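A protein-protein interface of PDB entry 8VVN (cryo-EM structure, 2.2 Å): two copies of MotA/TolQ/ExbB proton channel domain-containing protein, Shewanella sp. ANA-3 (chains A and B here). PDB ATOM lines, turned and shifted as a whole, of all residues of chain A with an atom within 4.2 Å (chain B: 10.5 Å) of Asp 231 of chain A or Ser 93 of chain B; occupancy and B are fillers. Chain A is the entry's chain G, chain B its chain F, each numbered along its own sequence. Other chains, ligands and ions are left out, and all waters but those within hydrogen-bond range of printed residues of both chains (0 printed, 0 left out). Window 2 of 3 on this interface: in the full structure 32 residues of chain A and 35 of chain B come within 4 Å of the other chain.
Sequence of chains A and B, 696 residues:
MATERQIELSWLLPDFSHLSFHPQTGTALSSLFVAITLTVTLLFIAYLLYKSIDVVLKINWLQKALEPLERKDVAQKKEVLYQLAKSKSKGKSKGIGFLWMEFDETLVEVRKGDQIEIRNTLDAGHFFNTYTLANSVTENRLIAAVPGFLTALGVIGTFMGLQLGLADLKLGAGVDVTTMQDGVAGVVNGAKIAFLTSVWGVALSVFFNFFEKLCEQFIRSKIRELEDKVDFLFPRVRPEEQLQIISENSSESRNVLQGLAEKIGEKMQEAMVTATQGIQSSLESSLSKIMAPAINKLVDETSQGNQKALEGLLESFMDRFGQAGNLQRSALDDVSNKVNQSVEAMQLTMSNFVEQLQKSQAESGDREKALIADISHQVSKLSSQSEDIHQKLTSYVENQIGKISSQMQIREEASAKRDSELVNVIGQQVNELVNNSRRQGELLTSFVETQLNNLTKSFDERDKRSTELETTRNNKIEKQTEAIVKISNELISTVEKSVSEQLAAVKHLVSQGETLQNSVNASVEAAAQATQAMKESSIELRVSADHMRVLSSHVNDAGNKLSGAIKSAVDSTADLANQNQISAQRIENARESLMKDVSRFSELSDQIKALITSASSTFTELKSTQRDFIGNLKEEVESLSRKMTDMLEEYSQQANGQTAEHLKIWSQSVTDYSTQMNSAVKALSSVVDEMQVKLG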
ATOM      1  N   ASP A 123      22.634  21.008 -22.669  1.00  0.00           N
ATOM      2  CA  ASP A 123      21.187  21.009 -22.844  1.00  0.00           C
ATOM      3  C   ASP A 123      20.662  19.586 -23.018  1.00  0.00           C
ATOM      4  O   ASP A 123      21.371  18.687 -23.477  1.00  0.00           O
ATOM      5  CB  ASP A 123      20.797  21.869 -24.044  1.00  0.00           C
ATOM      6  CG  ASP A 123      19.296  22.022 -24.189  1.00  0.00           C
ATOM      7  OD1 ASP A 123      18.696  22.775 -23.394  1.00  0.00           O
ATOM      8  OD2 ASP A 123      18.715  21.388 -25.096  1.00  0.00           O
ATOM      9  N   ALA A 124      19.394  19.390 -22.646  1.00  0.00           N
ATOM     10  CA  ALA A 124      18.774  18.071 -22.692  1.00  0.00           C
ATOM     11  C   ALA A 124      18.503  17.583 -24.108  1.00  0.00           C
ATOM     12  O   ALA A 124      18.139  16.415 -24.278  1.00  0.00           O
ATOM     13  CB  ALA A 124      17.468  18.075 -21.897  1.00  0.00           C
ATOM     14  N   GLU A 227      11.780  16.848 -23.040  1.00  0.00           N
ATOM     15  CA  GLU A 227      12.682  17.993 -23.103  1.00  0.00           C
ATOM     16  C   GLU A 227      12.213  19.113 -22.186  1.00  0.00           C
ATOM     17  O   GLU A 227      13.023  19.742 -21.497  1.00  0.00           O
ATOM     18  CB  GLU A 227      12.782  18.495 -24.542  1.00  0.00           C
ATOM     19  CG  GLU A 227      13.813  17.790 -25.390  1.00  0.00           C
ATOM     20  CD  GLU A 227      14.251  18.634 -26.566  1.00  0.00           C
ATOM     21  OE1 GLU A 227      15.469  18.826 -26.744  1.00  0.00           O
ATOM     22  OE2 GLU A 227      13.372  19.108 -27.317  1.00  0.00           O
ATOM     23  N   ASP A 228      10.906  19.375 -22.163  1.00  0.00           N
ATOM     24  CA  ASP A 228      10.381  20.426 -21.301  1.00  0.00           C
ATOM     25  C   ASP A 228      10.456  20.033 -19.831  1.00  0.00           C
ATOM     26  O   ASP A 228      10.905  20.826 -18.997  1.00  0.00           O
ATOM     27  CB  ASP A 228       8.943  20.754 -21.696  1.00  0.00           C
ATOM     28  CG  ASP A 228       8.855  21.442 -23.043  1.00  0.00           C
ATOM     29  OD1 ASP A 228       9.899  21.925 -23.531  1.00  0.00           O
ATOM     30  OD2 ASP A 228       7.744  21.502 -23.612  1.00  0.00           O
ATOM     31  N   LYS A 229      10.025  18.816 -19.495  1.00  0.00           N
ATOM     32  CA  LYS A 229       9.936  18.430 -18.089  1.00  0.00           C
ATOM     33  C   LYS A 229      11.314  18.203 -17.481  1.00  0.00           C
ATOM     34  O   LYS A 229      11.575  18.627 -16.350  1.00  0.00           O
ATOM     35  CB  LYS A 229       9.072  17.179 -17.940  1.00  0.00           C
ATOM     36  CG  LYS A 229       8.906  16.723 -16.504  1.00  0.00           C
ATOM     37  CD  LYS A 229       8.055  17.706 -15.715  1.00  0.00           C
ATOM     38  CE  LYS A 229       7.793  17.206 -14.305  1.00  0.00           C
ATOM     39  NZ  LYS A 229       7.017  18.189 -13.498  1.00  0.00           N
ATOM     40  N   VAL A 230      12.204  17.529 -18.211  1.00  0.00           N
ATOM     41  CA  VAL A 230      13.538  17.252 -17.687  1.00  0.00           C
ATOM     42  C   VAL A 230      14.322  18.542 -17.484  1.00  0.00           C
ATOM     43  O   VAL A 230      14.970  18.729 -16.447  1.00  0.00           O
ATOM     44  CB  VAL A 230      14.279  16.275 -18.615  1.00  0.00           C
ATOM     45  CG1 VAL A 230      15.687  16.075 -18.138  1.00  0.00           C
ATOM     46  CG2 VAL A 230      13.557  14.942 -18.652  1.00  0.00           C
ATOM     47  N   ASP A 231      14.281  19.448 -18.461  1.00  0.00           N
ATOM     48  CA  ASP A 231      15.021  20.700 -18.326  1.00  0.00           C
ATOM     49  C   ASP A 231      14.391  21.626 -17.294  1.00  0.00           C
ATOM     50  O   ASP A 231      15.101  22.418 -16.665  1.00  0.00           O
ATOM     51  CB  ASP A 231      15.128  21.402 -19.676  1.00  0.00           C
ATOM     52  CG  ASP A 231      16.455  21.148 -20.360  1.00  0.00           C
ATOM     53  OD1 ASP A 231      17.300  20.442 -19.770  1.00  0.00           O
ATOM     54  OD2 ASP A 231      16.655  21.652 -21.484  1.00  0.00           O
ATOM     55  N   PHE A 232      13.070  21.559 -17.119  1.00  0.00           N
ATOM     56  CA  PHE A 232      12.432  22.350 -16.071  1.00  0.00           C
ATOM     57  C   PHE A 232      12.912  21.917 -14.693  1.00  0.00           C
ATOM     58  O   PHE A 232      13.231  22.759 -13.845  1.00  0.00           O
ATOM     59  CB  PHE A 232      10.911  22.231 -16.174  1.00  0.00           C
ATOM     60  CG  PHE A 232      10.187  22.539 -14.895  1.00  0.00           C
ATOM     61  CD1 PHE A 232       9.491  21.548 -14.222  1.00  0.00           C
ATOM     62  CD2 PHE A 232      10.196  23.820 -14.368  1.00  0.00           C
ATOM     63  CE1 PHE A 232       8.822  21.828 -13.046  1.00  0.00           C
ATOM     64  CE2 PHE A 232       9.527  24.107 -13.194  1.00  0.00           C
ATOM     65  CZ  PHE A 232       8.839  23.108 -12.532  1.00  0.00           C
ATOM     66  N   LEU A 233      12.981  20.607 -14.455  1.00  0.00           N
ATOM     67  CA  LEU A 233      13.447  20.102 -13.170  1.00  0.00           C
ATOM     68  C   LEU A 233      14.962  20.188 -13.034  1.00  0.00           C
ATOM     69  O   LEU A 233      15.472  20.295 -11.914  1.00  0.00           O
ATOM     70  CB  LEU A 233      12.985  18.658 -12.975  1.00  0.00           C
ATOM     71  CG  LEU A 233      11.478  18.431 -12.847  1.00  0.00           C
ATOM     72  CD1 LEU A 233      11.174  16.946 -12.801  1.00  0.00           C
ATOM     73  CD2 LEU A 233      10.929  19.127 -11.615  1.00  0.00           C
ATOM     74  N   PHE A 234      15.693  20.134 -14.147  1.00  0.00           N
ATOM     75  CA  PHE A 234      17.155  20.155 -14.137  1.00  0.00           C
ATOM     76  C   PHE A 234      17.648  21.241 -15.082  1.00  0.00           C
ATOM     77  O   PHE A 234      17.969  20.966 -16.246  1.00  0.00           O
ATOM     78  CB  PHE A 234      17.745  18.800 -14.528  1.00  0.00           C
ATOM     79  CG  PHE A 234      17.478  17.697 -13.539  1.00  0.00           C
ATOM     80  CD1 PHE A 234      18.527  17.074 -12.886  1.00  0.00           C
ATOM     81  CD2 PHE A 234      16.191  17.246 -13.297  1.00  0.00           C
ATOM     82  CE1 PHE A 234      18.296  16.055 -11.984  1.00  0.00           C
ATOM     83  CE2 PHE A 234      15.953  16.228 -12.398  1.00  0.00           C
ATOM     84  CZ  PHE A 234      17.007  15.630 -11.741  1.00  0.00           C
ATOM     85  N   PRO A 235      17.719  22.499 -14.619  1.00  0.00           N
ATOM     86  CA  PRO A 235      18.230  23.611 -15.429  1.00  0.00           C
ATOM     87  C   PRO A 235      19.677  23.407 -15.867  1.00  0.00           C
ATOM     88  O   PRO A 235      19.915  23.127 -17.041  1.00  0.00           O
ATOM     89  CB  PRO A 235      18.120  24.806 -14.486  1.00  0.00           C
ATOM     90  CG  PRO A 235      17.051  24.436 -13.531  1.00  0.00           C
ATOM     91  CD  PRO A 235      17.182  22.961 -13.328  1.00  0.00           C
ATOM     92  N   LYS B  58       7.295  34.704 -31.052  1.00  0.00           N
ATOM     93  CA  LYS B  58       8.631  34.626 -30.468  1.00  0.00           C
ATOM     94  C   LYS B  58       9.569  35.634 -31.120  1.00  0.00           C
ATOM     95  O   LYS B  58      10.318  36.338 -30.435  1.00  0.00           O
ATOM     96  CB  LYS B  58       9.190  33.211 -30.609  1.00  0.00           C
ATOM     97  CG  LYS B  58       8.463  32.158 -29.805  1.00  0.00           C
ATOM     98  CD  LYS B  58       9.052  30.777 -30.056  1.00  0.00           C
ATOM     99  CE  LYS B  58       9.315  30.547 -31.532  1.00  0.00           C
ATOM    100  NZ  LYS B  58       9.595  29.120 -31.837  1.00  0.00           N
ATOM    101  N   ALA B  85      14.751  38.847 -20.511  1.00  0.00           N
ATOM    102  CA  ALA B  85      14.577  37.501 -21.045  1.00  0.00           C
ATOM    103  C   ALA B  85      14.039  36.554 -19.978  1.00  0.00           C
ATOM    104  O   ALA B  85      13.173  35.719 -20.262  1.00  0.00           O
ATOM    105  CB  ALA B  85      15.894  36.987 -21.621  1.00  0.00           C
ATOM    106  N   LYS B  86      14.539  36.669 -18.742  1.00  0.00           N
ATOM    107  CA  LYS B  86      13.968  35.907 -17.632  1.00  0.00           C
ATOM    108  C   LYS B  86      12.508  36.262 -17.389  1.00  0.00           C
ATOM    109  O   LYS B  86      11.755  35.443 -16.849  1.00  0.00           O
ATOM    110  CB  LYS B  86      14.764  36.143 -16.345  1.00  0.00           C
ATOM    111  CG  LYS B  86      16.210  35.685 -16.360  1.00  0.00           C
ATOM    112  CD  LYS B  86      16.299  34.179 -16.511  1.00  0.00           C
ATOM    113  CE  LYS B  86      15.838  33.458 -15.256  1.00  0.00           C
ATOM    114  NZ  LYS B  86      16.000  31.981 -15.382  1.00  0.00           N
ATOM    115  N   LYS B  88       9.883  36.673 -19.341  1.00  0.00           N
ATOM    116  CA  LYS B  88       8.902  35.873 -20.060  1.00  0.00           C
ATOM    117  C   LYS B  88       9.229  34.381 -20.051  1.00  0.00           C
ATOM    118  O   LYS B  88       8.370  33.567 -20.407  1.00  0.00           O
ATOM    119  CB  LYS B  88       8.780  36.375 -21.509  1.00  0.00           C
ATOM    120  CG  LYS B  88       7.743  35.647 -22.362  1.00  0.00           C
ATOM    121  CD  LYS B  88       7.580  36.270 -23.733  1.00  0.00           C
ATOM    122  CE  LYS B  88       8.774  35.965 -24.616  1.00  0.00           C
ATOM    123  NZ  LYS B  88       8.565  36.471 -25.995  1.00  0.00           N
ATOM    124  N   SER B  89      10.417  33.997 -19.591  1.00  0.00           N
ATOM    125  CA  SER B  89      10.938  32.644 -19.779  1.00  0.00           C
ATOM    126  C   SER B  89      10.703  31.748 -18.570  1.00  0.00           C
ATOM    127  O   SER B  89      11.576  30.951 -18.214  1.00  0.00           O
ATOM    128  CB  SER B  89      12.424  32.695 -20.120  1.00  0.00           C
ATOM    129  OG  SER B  89      12.868  31.452 -20.634  1.00  0.00           O
ATOM    130  N   LYS B  90       9.551  31.856 -17.910  1.00  0.00           N
ATOM    131  CA  LYS B  90       9.238  30.946 -16.810  1.00  0.00           C
ATOM    132  C   LYS B  90       9.121  29.549 -17.400  1.00  0.00           C
ATOM    133  O   LYS B  90       8.099  29.194 -17.993  1.00  0.00           O
ATOM    134  CB  LYS B  90       7.938  31.335 -16.113  1.00  0.00           C
ATOM    135  CG  LYS B  90       8.045  32.437 -15.073  1.00  0.00           C
ATOM    136  CD  LYS B  90       8.227  33.780 -15.745  1.00  0.00           C
ATOM    137  CE  LYS B  90       6.936  34.152 -16.457  1.00  0.00           C
ATOM    138  NZ  LYS B  90       6.966  35.483 -17.110  1.00  0.00           N
ATOM    139  N   GLY B  91      10.157  28.737 -17.225  1.00  0.00           N
ATOM    140  CA  GLY B  91      10.251  27.512 -17.990  1.00  0.00           C
ATOM    141  C   GLY B  91      10.700  27.819 -19.403  1.00  0.00           C
ATOM    142  O   GLY B  91      11.799  28.353 -19.597  1.00  0.00           O
ATOM    143  N   LYS B  92       9.860  27.512 -20.391  1.00  0.00           N
ATOM    144  CA  LYS B  92      10.152  27.774 -21.802  1.00  0.00           C
ATOM    145  C   LYS B  92      11.527  27.217 -22.180  1.00  0.00           C
ATOM    146  O   LYS B  92      12.475  27.945 -22.471  1.00  0.00           O
ATOM    147  CB  LYS B  92      10.051  29.271 -22.123  1.00  0.00           C
ATOM    148  CG  LYS B  92       8.633  29.790 -22.335  1.00  0.00           C
ATOM    149  CD  LYS B  92       7.854  29.887 -21.037  1.00  0.00           C
ATOM    150  CE  LYS B  92       6.481  30.493 -21.252  1.00  0.00           C
ATOM    151  NZ  LYS B  92       5.675  30.479 -20.001  1.00  0.00           N
ATOM    152  N   SER B  93      11.597  25.884 -22.146  1.00  0.00           N
ATOM    153  CA  SER B  93      12.868  25.186 -22.321  1.00  0.00           C
ATOM    154  C   SER B  93      13.575  25.584 -23.609  1.00  0.00           C
ATOM    155  O   SER B  93      14.810  25.611 -23.653  1.00  0.00           O
ATOM    156  CB  SER B  93      12.636  23.674 -22.296  1.00  0.00           C
ATOM    157  OG  SER B  93      13.844  22.977 -22.055  1.00  0.00           O
ATOM    158  N   LYS B  94      12.824  25.889 -24.664  1.00  0.00           N
ATOM    159  CA  LYS B  94      13.416  26.272 -25.940  1.00  0.00           C
ATOM    160  C   LYS B  94      12.658  27.441 -26.563  1.00  0.00           C
ATOM    161  O   LYS B  94      12.508  27.532 -27.786  1.00  0.00           O
ATOM    162  CB  LYS B  94      13.486  25.070 -26.883  1.00  0.00           C
ATOM    163  CG  LYS B  94      12.144  24.506 -27.315  1.00  0.00           C
ATOM    164  CD  LYS B  94      12.340  23.292 -28.205  1.00  0.00           C
ATOM    165  CE  LYS B  94      11.016  22.713 -28.669  1.00  0.00           C
ATOM    166  NZ  LYS B  94      11.229  21.522 -29.534  1.00  0.00           N
ATOM    167  N   GLY B  95      12.192  28.367 -25.727  1.00  0.00           N
ATOM    168  CA  GLY B  95      11.525  29.558 -26.207  1.00  0.00           C
ATOM    169  C   GLY B  95      12.502  30.632 -26.647  1.00  0.00           C
ATOM    170  O   GLY B  95      13.721  30.463 -26.628  1.00  0.00           O
ATOM    171  N   ILE B  96      11.938  31.768 -27.065  1.00  0.00           N
ATOM    172  CA  ILE B  96      12.772  32.887 -27.496  1.00  0.00           C
ATOM    173  C   ILE B  96      13.531  33.480 -26.314  1.00  0.00           C
ATOM    174  O   ILE B  96      14.680  33.916 -26.457  1.00  0.00           O
ATOM    175  CB  ILE B  96      11.924  33.944 -28.230  1.00  0.00           C
ATOM    176  CG1 ILE B  96      12.831  34.950 -28.942  1.00  0.00           C
ATOM    177  CG2 ILE B  96      10.967  34.649 -27.284  1.00  0.00           C
ATOM    178  CD1 ILE B  96      13.640  34.353 -30.064  1.00  0.00           C
ATOM    179  N   GLY B  97      12.910  33.508 -25.133  1.00  0.00           N
ATOM    180  CA  GLY B  97      13.623  33.959 -23.950  1.00  0.00           C
ATOM    181  C   GLY B  97      14.818  33.082 -23.633  1.00  0.00           C
ATOM    182  O   GLY B  97      15.869  33.574 -23.218  1.00  0.00           O
ATOM    183  N   PHE B  98      14.672  31.771 -23.831  1.00  0.00           N
ATOM    184  CA  PHE B  98      15.785  30.855 -23.610  1.00  0.00           C
ATOM    185  C   PHE B  98      16.851  31.018 -24.688  1.00  0.00           C
ATOM    186  O   PHE B  98      18.047  30.886 -24.409  1.00  0.00           O
ATOM    187  CB  PHE B  98      15.260  29.417 -23.552  1.00  0.00           C
ATOM    188  CG  PHE B  98      16.283  28.397 -23.120  1.00  0.00           C
ATOM    189  CD1 PHE B  98      17.323  28.020 -23.954  1.00  0.00           C
ATOM    190  CD2 PHE B  98      16.201  27.821 -21.863  1.00  0.00           C
ATOM    191  CE1 PHE B  98      18.255  27.087 -23.545  1.00  0.00           C
ATOM    192  CE2 PHE B  98      17.132  26.886 -21.451  1.00  0.00           C
ATOM    193  CZ  PHE B  98      18.159  26.520 -22.293  1.00  0.00           C
ATOM    194  N   LEU B  99      16.440  31.301 -25.927  1.00  0.00           N
ATOM    195  CA  LEU B  99      17.415  31.490 -26.994  1.00  0.00           C
ATOM    196  C   LEU B  99      18.299  32.703 -26.737  1.00  0.00           C
ATOM    197  O   LEU B  99      19.483  32.695 -27.091  1.00  0.00           O
ATOM    198  CB  LEU B  99      16.707  31.619 -28.341  1.00  0.00           C
ATOM    199  CG  LEU B  99      16.197  30.310 -28.942  1.00  0.00           C
ATOM    200  CD1 LEU B  99      15.699  30.542 -30.349  1.00  0.00           C
ATOM    201  CD2 LEU B  99      17.289  29.254 -28.931  1.00  0.00           C
ATOM    202  N   TRP B 100      17.743  33.755 -26.133  1.00  0.00           N
ATOM    203  CA  TRP B 100      18.567  34.885 -25.721  1.00  0.00           C
ATOM    204  C   TRP B 100      19.512  34.507 -24.589  1.00  0.00           C
ATOM    205  O   TRP B 100      20.570  35.129 -24.439  1.00  0.00           O
ATOM    206  CB  TRP B 100      17.688  36.060 -25.301  1.00  0.00           C
ATOM    207  CG  TRP B 100      18.374  37.391 -25.391  1.00  0.00           C
ATOM    208  CD1 TRP B 100      18.510  38.310 -24.391  1.00  0.00           C
ATOM    209  CD2 TRP B 100      19.004  37.963 -26.545  1.00  0.00           C
ATOM    210  NE1 TRP B 100      19.192  39.411 -24.847  1.00  0.00           N
ATOM    211  CE2 TRP B 100      19.507  39.223 -26.167  1.00  0.00           C
ATOM    212  CE3 TRP B 100      19.195  37.531 -27.862  1.00  0.00           C
ATOM    213  CZ2 TRP B 100      20.185  40.053 -27.054  1.00  0.00           C
ATOM    214  CZ3 TRP B 100      19.871  38.356 -28.741  1.00  0.00           C
ATOM    215  CH2 TRP B 100      20.356  39.602 -28.335  1.00  0.00           C
ATOM    216  N   MET B 101      19.151  33.508 -23.781  1.00  0.00           N
ATOM    217  CA  MET B 101      20.013  33.099 -22.678  1.00  0.00           C
ATOM    218  C   MET B 101      21.357  32.614 -23.201  1.00  0.00           C
ATOM    219  O   MET B 101      22.391  33.248 -22.973  1.00  0.00           O
ATOM    220  CB  MET B 101      19.348  31.994 -21.859  1.00  0.00           C
ATOM    221  CG  MET B 101      18.011  32.358 -21.264  1.00  0.00           C
ATOM    222  SD  MET B 101      18.017  33.711 -20.089  1.00  0.00           S
ATOM    223  CE  MET B 101      16.252  33.922 -19.914  1.00  0.00           C
ATOM    224  N   GLU B 102      21.348  31.501 -23.943  1.00  0.00           N
ATOM    225  CA  GLU B 102      22.592  30.895 -24.410  1.00  0.00           C
ATOM    226  C   GLU B 102      23.422  31.865 -25.238  1.00  0.00           C
ATOM    227  O   GLU B 102      24.655  31.784 -25.234  1.00  0.00           O
ATOM    228  CB  GLU B 102      22.293  29.637 -25.224  1.00  0.00           C
ATOM    229  CG  GLU B 102      21.701  28.497 -24.418  1.00  0.00           C
ATOM    230  CD  GLU B 102      21.407  27.278 -25.270  1.00  0.00           C
ATOM    231  OE1 GLU B 102      21.547  27.367 -26.507  1.00  0.00           O
ATOM    232  OE2 GLU B 102      21.038  26.230 -24.702  1.00  0.00           O
ATOM    233  N   THR B 132      15.900  26.634 -34.490  1.00  0.00           N
ATOM    234  CA  THR B 132      15.658  27.088 -33.128  1.00  0.00           C
ATOM    235  C   THR B 132      14.417  27.961 -32.994  1.00  0.00           C
ATOM    236  O   THR B 132      13.987  28.225 -31.866  1.00  0.00           O
ATOM    237  CB  THR B 132      16.876  27.854 -32.605  1.00  0.00           C
ATOM    238  OG1 THR B 132      17.144  28.970 -33.462  1.00  0.00           O
ATOM    239  CG2 THR B 132      18.092  26.947 -32.573  1.00  0.00           C
ATOM    240  N   ASN B 135      11.234  25.219 -36.131  1.00  0.00           N
ATOM    241  CA  ASN B 135      11.426  23.806 -36.442  1.00  0.00           C
ATOM    242  C   ASN B 135      10.108  23.057 -36.560  1.00  0.00           C
ATOM    243  O   ASN B 135      10.072  21.980 -37.163  1.00  0.00           O
ATOM    244  CB  ASN B 135      12.295  23.139 -35.377  1.00  0.00           C
ATOM    245  CG  ASN B 135      11.572  22.982 -34.054  1.00  0.00           C
ATOM    246  OD1 ASN B 135      11.036  23.946 -33.510  1.00  0.00           O
ATOM    247  ND2 ASN B 135      11.551  21.762 -33.532  1.00  0.00           N
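Hydrophobic or aromatic side chains of chain B that line the printed part of chain A: Phe 98.
Along chain A the printed residues that touch a printed residue of chain B span positions 123 to 231.
Among the printed residues, 5 pairs touch across the chains.
Among the printed residues, Asp or Glu carboxylates within 4 Å of a Lys or Arg side-chain nitrogen of the other chain: Glu 227 of chain A with Lys 94 of chain B (3.9 Å).
Asp 123 of chain A touches just one residue of chain B: Phe 98 (3.9 Å).
Of the printed residues of chain B, Glu 227 of chain A touches Ser 93 (3.4 Å) and Lys 94 (3.9 Å).
Of chain B, only Ser 93 comes within 4 Å of Asp 228 of chain A.
No residue of chain B comes within 4 Å of Val 230 of chain A.
Asp 231 of chain A touches just one residue of chain B: Ser 93 (3.1 Å).
Phe 234 of chain A touches none of the printed residues of chain B.
No residue of chain B comes within 4 Å of Pro 235 of chain A.
Gly 91 of chain B touches none of the printed residues of chain A.
Of the printed residues of chain A, Ser 93 of chain B touches Glu 227, Asp 228 and Asp 231.
Of the printed residues of chain A, Lys 94 of chain B touches Glu 227 (3.9 Å).
Of the printed residues of chain A, Phe 98 of chain B touches Asp 123 (3.9 Å).
The nearest residue of chain B that does not touch Asp 231 of chain A is Phe 98 of chain B (5.2 Å).
The nearest printed residue of chain A that does not touch Ser 93 of chain B is Asp 123 of chain A (4.8 Å).
OG of Ser 93 of chain B is in hydrogen-bond range of O of Glu 227 of chain A, at 3.4 Å.
OD2 of Asp 231 of chain A lies close to OG of Ser 93 of chain B (3.2 Å).
NZ of Lys 94 of chain B lies within salt-bridge range of OE2 of Glu 227 of chain A (3.9 Å).
No position is printed for both chains.
Of the 5 pairs that touch across the chains among the printed residues, none has its exchanged pair printed and touching as well.
OD1 of Asp 123 of chain A touches CZ of Phe 98 of chain B (3.9 Å).
OD1 of Asp 228 of chain A touches CB of Ser 93 of chain B, 3.5 Å away.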
